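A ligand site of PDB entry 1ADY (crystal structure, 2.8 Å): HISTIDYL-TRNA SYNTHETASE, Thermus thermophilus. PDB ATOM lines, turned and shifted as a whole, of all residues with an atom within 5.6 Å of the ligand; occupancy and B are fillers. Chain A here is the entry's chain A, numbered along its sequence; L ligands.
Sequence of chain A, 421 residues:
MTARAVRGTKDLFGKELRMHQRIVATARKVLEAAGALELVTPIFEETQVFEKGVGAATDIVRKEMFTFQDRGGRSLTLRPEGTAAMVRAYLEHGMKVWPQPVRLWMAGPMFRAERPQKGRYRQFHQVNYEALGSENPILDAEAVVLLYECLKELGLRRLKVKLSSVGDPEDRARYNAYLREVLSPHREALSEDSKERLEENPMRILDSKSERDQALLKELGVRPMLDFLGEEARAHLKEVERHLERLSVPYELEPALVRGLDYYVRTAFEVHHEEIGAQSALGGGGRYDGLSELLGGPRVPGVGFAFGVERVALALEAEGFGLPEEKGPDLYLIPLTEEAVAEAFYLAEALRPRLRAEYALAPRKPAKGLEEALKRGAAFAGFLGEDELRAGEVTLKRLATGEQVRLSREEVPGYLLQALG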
ATOM      1  N   ILE A  60       2.550  20.061  19.753  1.00  0.00           N
ATOM      2  CA  ILE A  60       2.425  19.546  18.401  1.00  0.00           C
ATOM      3  C   ILE A  60       2.486  18.020  18.441  1.00  0.00           C
ATOM      4  O   ILE A  60       1.516  17.347  18.097  1.00  0.00           O
ATOM      5  CB  ILE A  60       3.561  20.098  17.496  1.00  0.00           C
ATOM      6  CG1 ILE A  60       3.498  21.628  17.473  1.00  0.00           C
ATOM      7  CG2 ILE A  60       3.445  19.536  16.101  1.00  0.00           C
ATOM      8  CD1 ILE A  60       4.605  22.276  16.681  1.00  0.00           C
ATOM      9  N   PRO A  80       3.319  18.421  10.056  1.00  0.00           N
ATOM     10  CA  PRO A  80       2.854  19.601  10.811  1.00  0.00           C
ATOM     11  C   PRO A  80       3.815  20.779  10.688  1.00  0.00           C
ATOM     12  O   PRO A  80       3.451  21.927  10.974  1.00  0.00           O
ATOM     13  CB  PRO A  80       2.828  19.071  12.247  1.00  0.00           C
ATOM     14  CG  PRO A  80       4.025  18.196  12.291  1.00  0.00           C
ATOM     15  CD  PRO A  80       3.986  17.460  10.953  1.00  0.00           C
ATOM     16  N   GLU A  81       5.040  20.492  10.239  1.00  0.00           N
ATOM     17  CA  GLU A  81       6.093  21.482  10.094  1.00  0.00           C
ATOM     18  C   GLU A  81       7.160  20.934   9.150  1.00  0.00           C
ATOM     19  O   GLU A  81       7.322  19.723   9.034  1.00  0.00           O
ATOM     20  CB  GLU A  81       6.652  21.832  11.489  1.00  0.00           C
ATOM     21  CG  GLU A  81       8.100  22.225  11.568  1.00  0.00           C
ATOM     22  CD  GLU A  81       9.005  21.046  11.829  1.00  0.00           C
ATOM     23  OE1 GLU A  81       8.573  20.074  12.474  1.00  0.00           O
ATOM     24  OE2 GLU A  81      10.170  21.097  11.399  1.00  0.00           O
ATOM     25  N   GLY A  82       7.909  21.823   8.496  1.00  0.00           N
ATOM     26  CA  GLY A  82       8.901  21.382   7.516  1.00  0.00           C
ATOM     27  C   GLY A  82      10.347  21.077   7.865  1.00  0.00           C
ATOM     28  O   GLY A  82      10.948  20.190   7.270  1.00  0.00           O
ATOM     29  N   THR A  83      10.931  21.806   8.804  1.00  0.00           N
ATOM     30  CA  THR A  83      12.333  21.612   9.167  1.00  0.00           C
ATOM     31  C   THR A  83      12.807  20.180   9.324  1.00  0.00           C
ATOM     32  O   THR A  83      13.743  19.750   8.651  1.00  0.00           O
ATOM     33  CB  THR A  83      12.663  22.348  10.458  1.00  0.00           C
ATOM     34  OG1 THR A  83      12.048  23.630  10.453  1.00  0.00           O
ATOM     35  CG2 THR A  83      14.157  22.477  10.614  1.00  0.00           C
ATOM     36  N   ARG A 112      -2.064  20.629  11.324  1.00  0.00           N
ATOM     37  CA  ARG A 112      -1.983  20.617  12.782  1.00  0.00           C
ATOM     38  C   ARG A 112      -3.369  20.357  13.351  1.00  0.00           C
ATOM     39  O   ARG A 112      -4.301  21.115  13.103  1.00  0.00           O
ATOM     40  CB  ARG A 112      -1.437  21.948  13.313  1.00  0.00           C
ATOM     41  CG  ARG A 112      -0.146  21.792  14.094  1.00  0.00           C
ATOM     42  CD  ARG A 112       1.050  22.256  13.297  1.00  0.00           C
ATOM     43  NE  ARG A 112       1.311  23.680  13.507  1.00  0.00           N
ATOM     44  CZ  ARG A 112       2.522  24.232  13.486  1.00  0.00           C
ATOM     45  NH1 ARG A 112       3.596  23.500  13.257  1.00  0.00           N
ATOM     46  NH2 ARG A 112       2.647  25.525  13.757  1.00  0.00           N
ATOM     47  N   GLU A 114      -5.305  20.998  15.757  1.00  0.00           N
ATOM     48  CA  GLU A 114      -5.690  21.842  16.875  1.00  0.00           C
ATOM     49  C   GLU A 114      -7.022  22.518  16.591  1.00  0.00           C
ATOM     50  O   GLU A 114      -7.389  22.717  15.428  1.00  0.00           O
ATOM     51  CB  GLU A 114      -4.611  22.889  17.147  1.00  0.00           C
ATOM     52  CG  GLU A 114      -4.496  23.973  16.097  1.00  0.00           C
ATOM     53  CD  GLU A 114      -3.152  24.682  16.123  1.00  0.00           C
ATOM     54  OE1 GLU A 114      -2.637  24.945  17.235  1.00  0.00           O
ATOM     55  OE2 GLU A 114      -2.612  24.946  15.039  1.00  0.00           O
ATOM     56  N   GLY A 119      -6.971  32.552  12.501  1.00  0.00           N
ATOM     57  CA  GLY A 119      -5.543  32.483  12.265  1.00  0.00           C
ATOM     58  C   GLY A 119      -5.054  31.067  12.427  1.00  0.00           C
ATOM     59  O   GLY A 119      -4.052  30.689  11.826  1.00  0.00           O
ATOM     60  N   ARG A 120      -5.751  30.266  13.228  1.00  0.00           N
ATOM     61  CA  ARG A 120      -5.366  28.877  13.438  1.00  0.00           C
ATOM     62  C   ARG A 120      -6.224  27.936  12.598  1.00  0.00           C
ATOM     63  O   ARG A 120      -7.386  27.702  12.912  1.00  0.00           O
ATOM     64  CB  ARG A 120      -5.473  28.496  14.917  1.00  0.00           C
ATOM     65  CG  ARG A 120      -4.485  29.215  15.806  1.00  0.00           C
ATOM     66  CD  ARG A 120      -4.536  28.673  17.211  1.00  0.00           C
ATOM     67  NE  ARG A 120      -3.690  29.441  18.122  1.00  0.00           N
ATOM     68  CZ  ARG A 120      -3.408  29.063  19.380  1.00  0.00           C
ATOM     69  NH1 ARG A 120      -3.869  27.910  19.875  1.00  0.00           N
ATOM     70  NH2 ARG A 120      -2.672  29.862  20.148  1.00  0.00           N
ATOM     71  N   TYR A 121      -5.659  27.469  11.479  1.00  0.00           N
ATOM     72  CA  TYR A 121      -6.354  26.556  10.596  1.00  0.00           C
ATOM     73  C   TYR A 121      -5.788  25.177  10.847  1.00  0.00           C
ATOM     74  O   TYR A 121      -4.681  25.047  11.385  1.00  0.00           O
ATOM     75  CB  TYR A 121      -6.086  26.915   9.138  1.00  0.00           C
ATOM     76  CG  TYR A 121      -6.506  28.303   8.740  1.00  0.00           C
ATOM     77  CD1 TYR A 121      -7.291  29.093   9.586  1.00  0.00           C
ATOM     78  CD2 TYR A 121      -6.148  28.812   7.509  1.00  0.00           C
ATOM     79  CE1 TYR A 121      -7.703  30.380   9.192  1.00  0.00           C
ATOM     80  CE2 TYR A 121      -6.554  30.077   7.109  1.00  0.00           C
ATOM     81  CZ  TYR A 121      -7.325  30.856   7.946  1.00  0.00           C
ATOM     82  OH  TYR A 121      -7.702  32.109   7.539  1.00  0.00           O
ATOM     83  N   PHE A 124      -2.956  24.687   6.812  1.00  0.00           N
ATOM     84  CA  PHE A 124      -2.483  26.001   6.415  1.00  0.00           C
ATOM     85  C   PHE A 124      -1.328  25.796   5.450  1.00  0.00           C
ATOM     86  O   PHE A 124      -0.941  24.665   5.157  1.00  0.00           O
ATOM     87  CB  PHE A 124      -2.042  26.800   7.645  1.00  0.00           C
ATOM     88  CG  PHE A 124      -1.139  26.033   8.574  1.00  0.00           C
ATOM     89  CD1 PHE A 124      -1.676  25.128   9.484  1.00  0.00           C
ATOM     90  CD2 PHE A 124       0.236  26.211   8.547  1.00  0.00           C
ATOM     91  CE1 PHE A 124      -0.842  24.409  10.348  1.00  0.00           C
ATOM     92  CE2 PHE A 124       1.073  25.505   9.397  1.00  0.00           C
ATOM     93  CZ  PHE A 124       0.530  24.595  10.302  1.00  0.00           C
ATOM     94  N   GLN A 126       2.657  27.340   4.335  1.00  0.00           N
ATOM     95  CA  GLN A 126       3.781  28.175   4.732  1.00  0.00           C
ATOM     96  C   GLN A 126       4.984  28.037   3.812  1.00  0.00           C
ATOM     97  O   GLN A 126       5.193  27.001   3.190  1.00  0.00           O
ATOM     98  CB  GLN A 126       4.210  27.876   6.173  1.00  0.00           C
ATOM     99  CG  GLN A 126       4.830  26.498   6.393  1.00  0.00           C
ATOM    100  CD  GLN A 126       5.238  26.233   7.848  1.00  0.00           C
ATOM    101  OE1 GLN A 126       4.557  26.661   8.785  1.00  0.00           O
ATOM    102  NE2 GLN A 126       6.351  25.523   8.033  1.00  0.00           N
ATOM    103  N   ASN A 128       8.889  27.839   3.478  1.00  0.00           N
ATOM    104  CA  ASN A 128       9.926  27.357   4.378  1.00  0.00           C
ATOM    105  C   ASN A 128      11.326  27.505   3.816  1.00  0.00           C
ATOM    106  O   ASN A 128      11.591  27.055   2.704  1.00  0.00           O
ATOM    107  CB  ASN A 128       9.644  25.882   4.698  1.00  0.00           C
ATOM    108  CG  ASN A 128      10.479  25.357   5.842  1.00  0.00           C
ATOM    109  OD1 ASN A 128      10.016  25.307   6.990  1.00  0.00           O
ATOM    110  ND2 ASN A 128      11.692  24.909   5.545  1.00  0.00           N
ATOM    111  N   TYR A 129      12.222  28.115   4.587  1.00  0.00           N
ATOM    112  CA  TYR A 129      13.614  28.316   4.184  1.00  0.00           C
ATOM    113  C   TYR A 129      14.557  27.616   5.168  1.00  0.00           C
ATOM    114  O   TYR A 129      14.329  27.671   6.372  1.00  0.00           O
ATOM    115  CB  TYR A 129      13.960  29.799   4.118  1.00  0.00           C
ATOM    116  CG  TYR A 129      15.438  30.046   3.981  1.00  0.00           C
ATOM    117  CD1 TYR A 129      16.103  29.802   2.784  1.00  0.00           C
ATOM    118  CD2 TYR A 129      16.183  30.526   5.060  1.00  0.00           C
ATOM    119  CE1 TYR A 129      17.484  30.005   2.659  1.00  0.00           C
ATOM    120  CE2 TYR A 129      17.556  30.728   4.946  1.00  0.00           C
ATOM    121  CZ  TYR A 129      18.199  30.473   3.749  1.00  0.00           C
ATOM    122  OH  TYR A 129      19.558  30.675   3.633  1.00  0.00           O
ATOM    123  N   GLU A 130      15.631  27.043   4.645  1.00  0.00           N
ATOM    124  CA  GLU A 130      16.615  26.304   5.433  1.00  0.00           C
ATOM    125  C   GLU A 130      18.047  26.517   4.938  1.00  0.00           C
ATOM    126  O   GLU A 130      18.286  26.654   3.736  1.00  0.00           O
ATOM    127  CB  GLU A 130      16.293  24.801   5.346  1.00  0.00           C
ATOM    128  CG  GLU A 130      16.021  24.106   6.666  1.00  0.00           C
ATOM    129  CD  GLU A 130      14.877  24.722   7.452  1.00  0.00           C
ATOM    130  OE1 GLU A 130      15.059  25.858   7.945  1.00  0.00           O
ATOM    131  OE2 GLU A 130      13.809  24.087   7.599  1.00  0.00           O
ATOM    132  N   ARG A 259      10.342  29.320  21.717  1.00  0.00           N
ATOM    133  CA  ARG A 259       9.726  28.994  20.459  1.00  0.00           C
ATOM    134  C   ARG A 259       8.814  27.787  20.688  1.00  0.00           C
ATOM    135  O   ARG A 259       8.868  27.171  21.765  1.00  0.00           O
ATOM    136  CB  ARG A 259      10.813  28.704  19.416  1.00  0.00           C
ATOM    137  CG  ARG A 259      10.387  28.994  17.996  1.00  0.00           C
ATOM    138  CD  ARG A 259      10.177  30.453  17.730  1.00  0.00           C
ATOM    139  NE  ARG A 259       9.089  30.688  16.780  1.00  0.00           N
ATOM    140  CZ  ARG A 259       9.022  30.183  15.545  1.00  0.00           C
ATOM    141  NH1 ARG A 259       9.987  29.415  15.069  1.00  0.00           N
ATOM    142  NH2 ARG A 259       8.014  30.514  14.756  1.00  0.00           N
ATOM    143  N   GLY A 260       7.959  27.477  19.723  1.00  0.00           N
ATOM    144  CA  GLY A 260       7.055  26.357  19.869  1.00  0.00           C
ATOM    145  C   GLY A 260       7.644  24.987  19.551  1.00  0.00           C
ATOM    146  O   GLY A 260       6.923  23.988  19.538  1.00  0.00           O
ATOM    147  N   LEU A 261       8.942  24.935  19.281  1.00  0.00           N
ATOM    148  CA  LEU A 261       9.597  23.681  18.946  1.00  0.00           C
ATOM    149  C   LEU A 261      10.867  23.476  19.759  1.00  0.00           C
ATOM    150  O   LEU A 261      11.641  24.405  19.965  1.00  0.00           O
ATOM    151  CB  LEU A 261       9.882  23.632  17.438  1.00  0.00           C
ATOM    152  CG  LEU A 261       8.640  23.807  16.545  1.00  0.00           C
ATOM    153  CD1 LEU A 261       8.308  25.284  16.357  1.00  0.00           C
ATOM    154  CD2 LEU A 261       8.894  23.176  15.191  1.00  0.00           C
ATOM    155  N   TYR A 263      13.625  21.636  19.009  1.00  0.00           N
ATOM    156  CA  TYR A 263      14.891  21.424  18.307  1.00  0.00           C
ATOM    157  C   TYR A 263      15.760  22.671  18.219  1.00  0.00           C
ATOM    158  O   TYR A 263      16.925  22.610  17.794  1.00  0.00           O
ATOM    159  CB  TYR A 263      14.664  20.801  16.919  1.00  0.00           C
ATOM    160  CG  TYR A 263      13.748  21.558  15.980  1.00  0.00           C
ATOM    161  CD1 TYR A 263      14.012  22.893  15.622  1.00  0.00           C
ATOM    162  CD2 TYR A 263      12.635  20.945  15.418  1.00  0.00           C
ATOM    163  CE1 TYR A 263      13.193  23.570  14.721  1.00  0.00           C
ATOM    164  CE2 TYR A 263      11.823  21.610  14.521  1.00  0.00           C
ATOM    165  CZ  TYR A 263      12.105  22.925  14.175  1.00  0.00           C
ATOM    166  OH  TYR A 263      11.300  23.584  13.273  1.00  0.00           O
ATOM    167  N   TYR A 264      15.195  23.803  18.636  1.00  0.00           N
ATOM    168  CA  TYR A 264      15.901  25.077  18.615  1.00  0.00           C
ATOM    169  C   TYR A 264      17.063  25.168  19.592  1.00  0.00           C
ATOM    170  O   TYR A 264      16.962  24.774  20.755  1.00  0.00           O
ATOM    171  CB  TYR A 264      14.946  26.228  18.899  1.00  0.00           C
ATOM    172  CG  TYR A 264      14.043  26.538  17.734  1.00  0.00           C
ATOM    173  CD1 TYR A 264      14.560  27.084  16.565  1.00  0.00           C
ATOM    174  CD2 TYR A 264      12.686  26.266  17.799  1.00  0.00           C
ATOM    175  CE1 TYR A 264      13.732  27.362  15.479  1.00  0.00           C
ATOM    176  CE2 TYR A 264      11.855  26.530  16.728  1.00  0.00           C
ATOM    177  CZ  TYR A 264      12.384  27.079  15.578  1.00  0.00           C
ATOM    178  OH  TYR A 264      11.539  27.365  14.524  1.00  0.00           O
ATOM    179  N   ALA A 281       2.021  36.405  14.809  1.00  0.00           N
ATOM    180  CA  ALA A 281       3.235  35.842  14.251  1.00  0.00           C
ATOM    181  C   ALA A 281       3.140  35.556  12.760  1.00  0.00           C
ATOM    182  O   ALA A 281       2.623  34.501  12.369  1.00  0.00           O
ATOM    183  CB  ALA A 281       3.606  34.573  15.016  1.00  0.00           C
ATOM    184  N   LEU A 282       3.632  36.469  11.932  1.00  0.00           N
ATOM    185  CA  LEU A 282       3.599  36.242  10.494  1.00  0.00           C
ATOM    186  C   LEU A 282       4.485  35.048  10.170  1.00  0.00           C
ATOM    187  O   LEU A 282       4.117  34.172   9.379  1.00  0.00           O
ATOM    188  CB  LEU A 282       4.103  37.468   9.727  1.00  0.00           C
ATOM    189  CG  LEU A 282       3.211  38.703   9.811  1.00  0.00           C
ATOM    190  CD1 LEU A 282       3.786  39.802   8.924  1.00  0.00           C
ATOM    191  CD2 LEU A 282       1.784  38.352   9.388  1.00  0.00           C
ATOM    192  N   GLY A 283       5.646  34.991  10.829  1.00  0.00           N
ATOM    193  CA  GLY A 283       6.569  33.897  10.607  1.00  0.00           C
ATOM    194  C   GLY A 283       7.563  33.763  11.745  1.00  0.00           C
ATOM    195  O   GLY A 283       7.686  34.666  12.576  1.00  0.00           O
ATOM    196  N   GLY A 284       8.277  32.641  11.779  1.00  0.00           N
ATOM    197  CA  GLY A 284       9.255  32.410  12.823  1.00  0.00           C
ATOM    198  C   GLY A 284      10.310  31.399  12.425  1.00  0.00           C
ATOM    199  O   GLY A 284      10.156  30.702  11.422  1.00  0.00           O
ATOM    200  N   GLY A 285      11.387  31.330  13.196  1.00  0.00           N
ATOM    201  CA  GLY A 285      12.457  30.399  12.889  1.00  0.00           C
ATOM    202  C   GLY A 285      13.574  30.500  13.896  1.00  0.00           C
ATOM    203  O   GLY A 285      13.448  31.185  14.908  1.00  0.00           O
ATOM    204  N   GLY A 286      14.680  29.823  13.600  1.00  0.00           N
ATOM    205  CA  GLY A 286      15.826  29.834  14.486  1.00  0.00           C
ATOM    206  C   GLY A 286      16.805  28.720  14.143  1.00  0.00           C
ATOM    207  O   GLY A 286      16.575  27.953  13.200  1.00  0.00           O
ATOM    208  N   TYR A 288      18.881  25.186  14.838  1.00  0.00           N
ATOM    209  CA  TYR A 288      18.429  23.910  15.372  1.00  0.00           C
ATOM    210  C   TYR A 288      19.457  22.796  15.218  1.00  0.00           C
ATOM    211  O   TYR A 288      19.134  21.687  14.781  1.00  0.00           O
ATOM    212  CB  TYR A 288      17.114  23.498  14.688  1.00  0.00           C
ATOM    213  CG  TYR A 288      17.161  23.630  13.172  1.00  0.00           C
ATOM    214  CD1 TYR A 288      17.711  22.614  12.391  1.00  0.00           C
ATOM    215  CD2 TYR A 288      16.748  24.799  12.542  1.00  0.00           C
ATOM    216  CE1 TYR A 288      17.864  22.761  11.019  1.00  0.00           C
ATOM    217  CE2 TYR A 288      16.895  24.966  11.159  1.00  0.00           C
ATOM    218  CZ  TYR A 288      17.455  23.939  10.411  1.00  0.00           C
ATOM    219  OH  TYR A 288      17.656  24.099   9.059  1.00  0.00           O
ATOM    220  N   VAL A 303      19.938  26.674  10.203  1.00  0.00           N
ATOM    221  CA  VAL A 303      19.079  27.797  10.574  1.00  0.00           C
ATOM    222  C   VAL A 303      18.019  27.914   9.492  1.00  0.00           C
ATOM    223  O   VAL A 303      18.224  27.461   8.351  1.00  0.00           O
ATOM    224  CB  VAL A 303      19.826  29.144  10.601  1.00  0.00           C
ATOM    225  CG1 VAL A 303      19.634  29.825  11.944  1.00  0.00           C
ATOM    226  CG2 VAL A 303      21.289  28.983  10.257  1.00  0.00           C
ATOM    227  N   GLY A 304      16.900  28.536   9.816  1.00  0.00           N
ATOM    228  CA  GLY A 304      15.847  28.715   8.835  1.00  0.00           C
ATOM    229  C   GLY A 304      14.589  29.322   9.427  1.00  0.00           C
ATOM    230  O   GLY A 304      14.522  29.568  10.631  1.00  0.00           O
ATOM    231  N   PHE A 305      13.576  29.502   8.592  1.00  0.00           N
ATOM    232  CA  PHE A 305      12.324  30.086   9.053  1.00  0.00           C
ATOM    233  C   PHE A 305      11.170  29.559   8.220  1.00  0.00           C
ATOM    234  O   PHE A 305      11.375  28.786   7.276  1.00  0.00           O
ATOM    235  CB  PHE A 305      12.378  31.610   8.948  1.00  0.00           C
ATOM    236  CG  PHE A 305      12.430  32.114   7.520  1.00  0.00           C
ATOM    237  CD1 PHE A 305      11.250  32.376   6.817  1.00  0.00           C
ATOM    238  CD2 PHE A 305      13.649  32.315   6.881  1.00  0.00           C
ATOM    239  CE1 PHE A 305      11.285  32.829   5.505  1.00  0.00           C
ATOM    240  CE2 PHE A 305      13.693  32.770   5.557  1.00  0.00           C
ATOM    241  CZ  PHE A 305      12.510  33.028   4.878  1.00  0.00           C
ATOM    242  N   ALA A 306       9.967  29.997   8.550  1.00  0.00           N
ATOM    243  CA  ALA A 306       8.762  29.611   7.855  1.00  0.00           C
ATOM    244  C   ALA A 306       7.650  30.580   8.232  1.00  0.00           C
ATOM    245  O   ALA A 306       7.454  30.877   9.407  1.00  0.00           O
ATOM    246  CB  ALA A 306       8.364  28.198   8.227  1.00  0.00           C
ATOM    247  N   PHE A 307       6.954  31.107   7.239  1.00  0.00           N
ATOM    248  CA  PHE A 307       5.866  32.038   7.514  1.00  0.00           C
ATOM    249  C   PHE A 307       4.543  31.549   6.923  1.00  0.00           C
ATOM    250  O   PHE A 307       4.511  30.963   5.838  1.00  0.00           O
ATOM    251  CB  PHE A 307       6.201  33.460   7.015  1.00  0.00           C
ATOM    252  CG  PHE A 307       6.309  33.586   5.518  1.00  0.00           C
ATOM    253  CD1 PHE A 307       5.171  33.792   4.741  1.00  0.00           C
ATOM    254  CD2 PHE A 307       7.552  33.581   4.882  1.00  0.00           C
ATOM    255  CE1 PHE A 307       5.270  33.984   3.360  1.00  0.00           C
ATOM    256  CE2 PHE A 307       7.651  33.783   3.510  1.00  0.00           C
ATOM    257  CZ  PHE A 307       6.509  33.986   2.758  1.00  0.00           C
ATOM    258  N   GLY A 308       3.461  31.801   7.654  1.00  0.00           N
ATOM    259  CA  GLY A 308       2.139  31.394   7.224  1.00  0.00           C
ATOM    260  C   GLY A 308       1.575  32.295   6.148  1.00  0.00           C
ATOM    261  O   GLY A 308       1.289  33.470   6.389  1.00  0.00           O
ATOM    262  N   GLU A 310      -1.313  32.421   4.912  1.00  0.00           N
ATOM    263  CA  GLU A 310      -2.616  32.943   5.292  1.00  0.00           C
ATOM    264  C   GLU A 310      -2.445  34.205   6.137  1.00  0.00           C
ATOM    265  O   GLU A 310      -3.042  35.246   5.853  1.00  0.00           O
ATOM    266  CB  GLU A 310      -3.436  31.901   6.053  1.00  0.00           C
ATOM    267  CG  GLU A 310      -3.956  30.743   5.204  1.00  0.00           C
ATOM    268  CD  GLU A 310      -2.967  29.595   5.053  1.00  0.00           C
ATOM    269  OE1 GLU A 310      -1.838  29.682   5.578  1.00  0.00           O
ATOM    270  OE2 GLU A 310      -3.330  28.588   4.402  1.00  0.00           O
ATOM    271  N   ARG A 311      -1.591  34.116   7.156  1.00  0.00           N
ATOM    272  CA  ARG A 311      -1.322  35.231   8.060  1.00  0.00           C
ATOM    273  C   ARG A 311      -0.827  36.409   7.219  1.00  0.00           C
ATOM    274  O   ARG A 311      -1.337  37.523   7.337  1.00  0.00           O
ATOM    275  CB  ARG A 311      -0.244  34.841   9.082  1.00  0.00           C
ATOM    276  CG  ARG A 311      -0.621  33.701  10.033  1.00  0.00           C
ATOM    277  CD  ARG A 311      -1.359  34.207  11.257  1.00  0.00           C
ATOM    278  NE  ARG A 311      -1.669  33.161  12.225  1.00  0.00           N
ATOM    279  CZ  ARG A 311      -0.769  32.560  13.018  1.00  0.00           C
ATOM    280  NH1 ARG A 311       0.519  32.897  12.962  1.00  0.00           N
ATOM    281  NH2 ARG A 311      -1.161  31.663  13.906  1.00  0.00           N
HETATM  282  P1  LIG L   1       6.128  27.588  13.821  1.00  0.00           P
HETATM  283  O1  LIG L   1       5.616  26.297  14.316  1.00  0.00           O
HETATM  284  O2  LIG L   1       6.320  28.629  14.863  1.00  0.00           O
HETATM  285  O3  LIG L   1       7.468  27.291  12.995  1.00  0.00           O
HETATM  286  O4  LIG L   1       5.126  28.280  12.791  1.00  0.00           O
HETATM  287  C1  LIG L   1       5.628  29.313  11.940  1.00  0.00           C
HETATM  288  C2  LIG L   1       4.497  30.072  11.257  1.00  0.00           C
HETATM  289  O5  LIG L   1       3.550  29.146  10.706  1.00  0.00           O
HETATM  290  C3  LIG L   1       3.699  30.907  12.239  1.00  0.00           C
HETATM  291  O6  LIG L   1       4.264  32.190  12.522  1.00  0.00           O
HETATM  292  C4  LIG L   1       2.427  31.098  11.440  1.00  0.00           C
HETATM  293  O7  LIG L   1       2.561  32.133  10.444  1.00  0.00           O
HETATM  294  C5  LIG L   1       2.251  29.735  10.776  1.00  0.00           C
HETATM  295  N1  LIG L   1       1.325  28.819  11.470  1.00  0.00           N
HETATM  296  C6  LIG L   1       1.616  27.938  12.449  1.00  0.00           C
HETATM  297  N2  LIG L   1       0.514  27.336  12.911  1.00  0.00           N
HETATM  298  C7  LIG L   1      -0.452  27.869  12.168  1.00  0.00           C
HETATM  299  C8  LIG L   1      -1.825  27.573  12.290  1.00  0.00           C
HETATM  300  N3  LIG L   1      -2.249  26.734  13.186  1.00  0.00           N
HETATM  301  N4  LIG L   1      -2.643  28.203  11.428  1.00  0.00           N
HETATM  302  C9  LIG L   1      -2.167  29.075  10.531  1.00  0.00           C
HETATM  303  N5  LIG L   1      -0.876  29.388  10.438  1.00  0.00           N
HETATM  304  C10 LIG L   1      -0.002  28.766  11.262  1.00  0.00           C
HETATM  305  C11 LIG L   1       7.946  26.171  12.229  1.00  0.00           C
HETATM  306  O8  LIG L   1       7.156  25.387  11.742  1.00  0.00           O
HETATM  307  C12 LIG L   1       9.443  25.940  12.045  1.00  0.00           C
HETATM  308  N6  LIG L   1       9.687  24.627  11.473  1.00  0.00           N
HETATM  309  C13 LIG L   1      10.067  27.031  11.159  1.00  0.00           C
HETATM  310  C14 LIG L   1      11.542  26.835  10.936  1.00  0.00           C
HETATM  311  C15 LIG L   1      12.246  26.549   9.818  1.00  0.00           C
HETATM  312  N7  LIG L   1      12.450  26.824  11.968  1.00  0.00           N
HETATM  313  C16 LIG L   1      13.640  26.506  11.499  1.00  0.00           C
HETATM  314  N8  LIG L   1      13.544  26.333  10.198  1.00  0.00           N
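OH of Tyr 263 is in hydrogen-bond range of N6 of the ligand (2.6 Å). The side-chain amide oxygen (OE1) of Gln 126 sits close to an oxygen (O5) of the ligand (3.3 Å). An oxygen (O1) of the ligand is in salt-bridge range of the guanidinium group of Arg 112 (3.1 Å). The side-chain carboxylate (OE2) of Glu 114 lies within hydrogen-bond range of a nitrogen (N3) of the ligand. The side-chain carboxylate (OE2) of Glu 81 lies within salt-bridge range of a nitrogen (N6) of the ligand. O of Gly 304 lies close to N8 of the ligand, 3.4 Å away. The backbone carbonyl oxygen (O) of Ala 281 lies within hydrogen-bond range of an oxygen (O6) of the ligand, 2.8 Å away. A nitrogen (N3) of the ligand sits at hydrogen-bond distance from the backbone carbonyl oxygen of Tyr 121 (3.5 Å). N of Gly 308 sits at hydrogen-bond distance from O7 of the ligand (3.0 Å). N8 of the ligand sits at hydrogen-bond distance from OE1 of Glu 130, 2.8 Å away. NH1 of Arg 311 lies close to O7 of the ligand. O of Leu 282 lies within hydrogen-bond range of O7 of the ligand (2.8 Å). The side-chain hydroxyl of Thr 83 sits at hydrogen-bond distance from a nitrogen (N6) of the ligand, 2.8 Å away. OH of Tyr 264 lies within hydrogen-bond range of N7 of the ligand, 2.8 Å away. The guanidinium group of Arg 259 is in salt-bridge range of an oxygen (O2) of the ligand (2.5 Å). A nitrogen (N4) of the ligand lies within hydrogen-bond range of the backbone NH (N) of Tyr 121 (3.1 Å).
NH1 of Arg 112 lies within hydrogen-bond range of O of Pro 80, 2.8 Å away. The side-chain hydroxyl (OH) of Tyr 288 sits close to the side-chain carboxylate (OE1) of Glu 130 (3.3 Å). O of Phe 305 sits at hydrogen-bond distance from N of Tyr 129. O of Gly 119 is in hydrogen-bond range of NE of Arg 311. The side-chain amide nitrogen (ND2) of Asn 128 sits at hydrogen-bond distance from the side-chain carboxylate (OE2) of Glu 130 (3.1 Å). The backbone NH (N) of Gly 308 is in hydrogen-bond range of the backbone carbonyl oxygen (O) of Leu 282, at 3.0 Å. The side-chain hydroxyl (OH) of Tyr 263 sits at hydrogen-bond distance from the side-chain hydroxyl (OG1) of Thr 83 (2.9 Å). O of Gly 304 is in hydrogen-bond range of N of Gly 286, 3.0 Å away.
The backbone carbonyl oxygen of Gly 119 sits close to a nitrogen (N4) of the ligand (2.9 Å). Arg 120 touches the ligand. CB of Phe 124 touches C9 of the ligand, 3.7 Å away. Asn 128 touches the ligand. Leu 261 touches the ligand (CD1 to O1, 3.5 Å). Gly 283 touches the ligand (CA to O6, 3.4 Å). Gly 284 touches the ligand (O to C13, 3.7 Å). CA of Gly 285 touches N7 of the ligand, 3.7 Å away. Gly 286 touches the ligand (O to C16, 3.7 Å). Tyr 288 touches the ligand. N of Phe 305 touches C15 of the ligand, at 3.5 Å. Ala 306 touches the ligand (O to C1, 3.5 Å). The nearest printed residue that does not touch the ligand is Phe 307 (4.1 Å).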
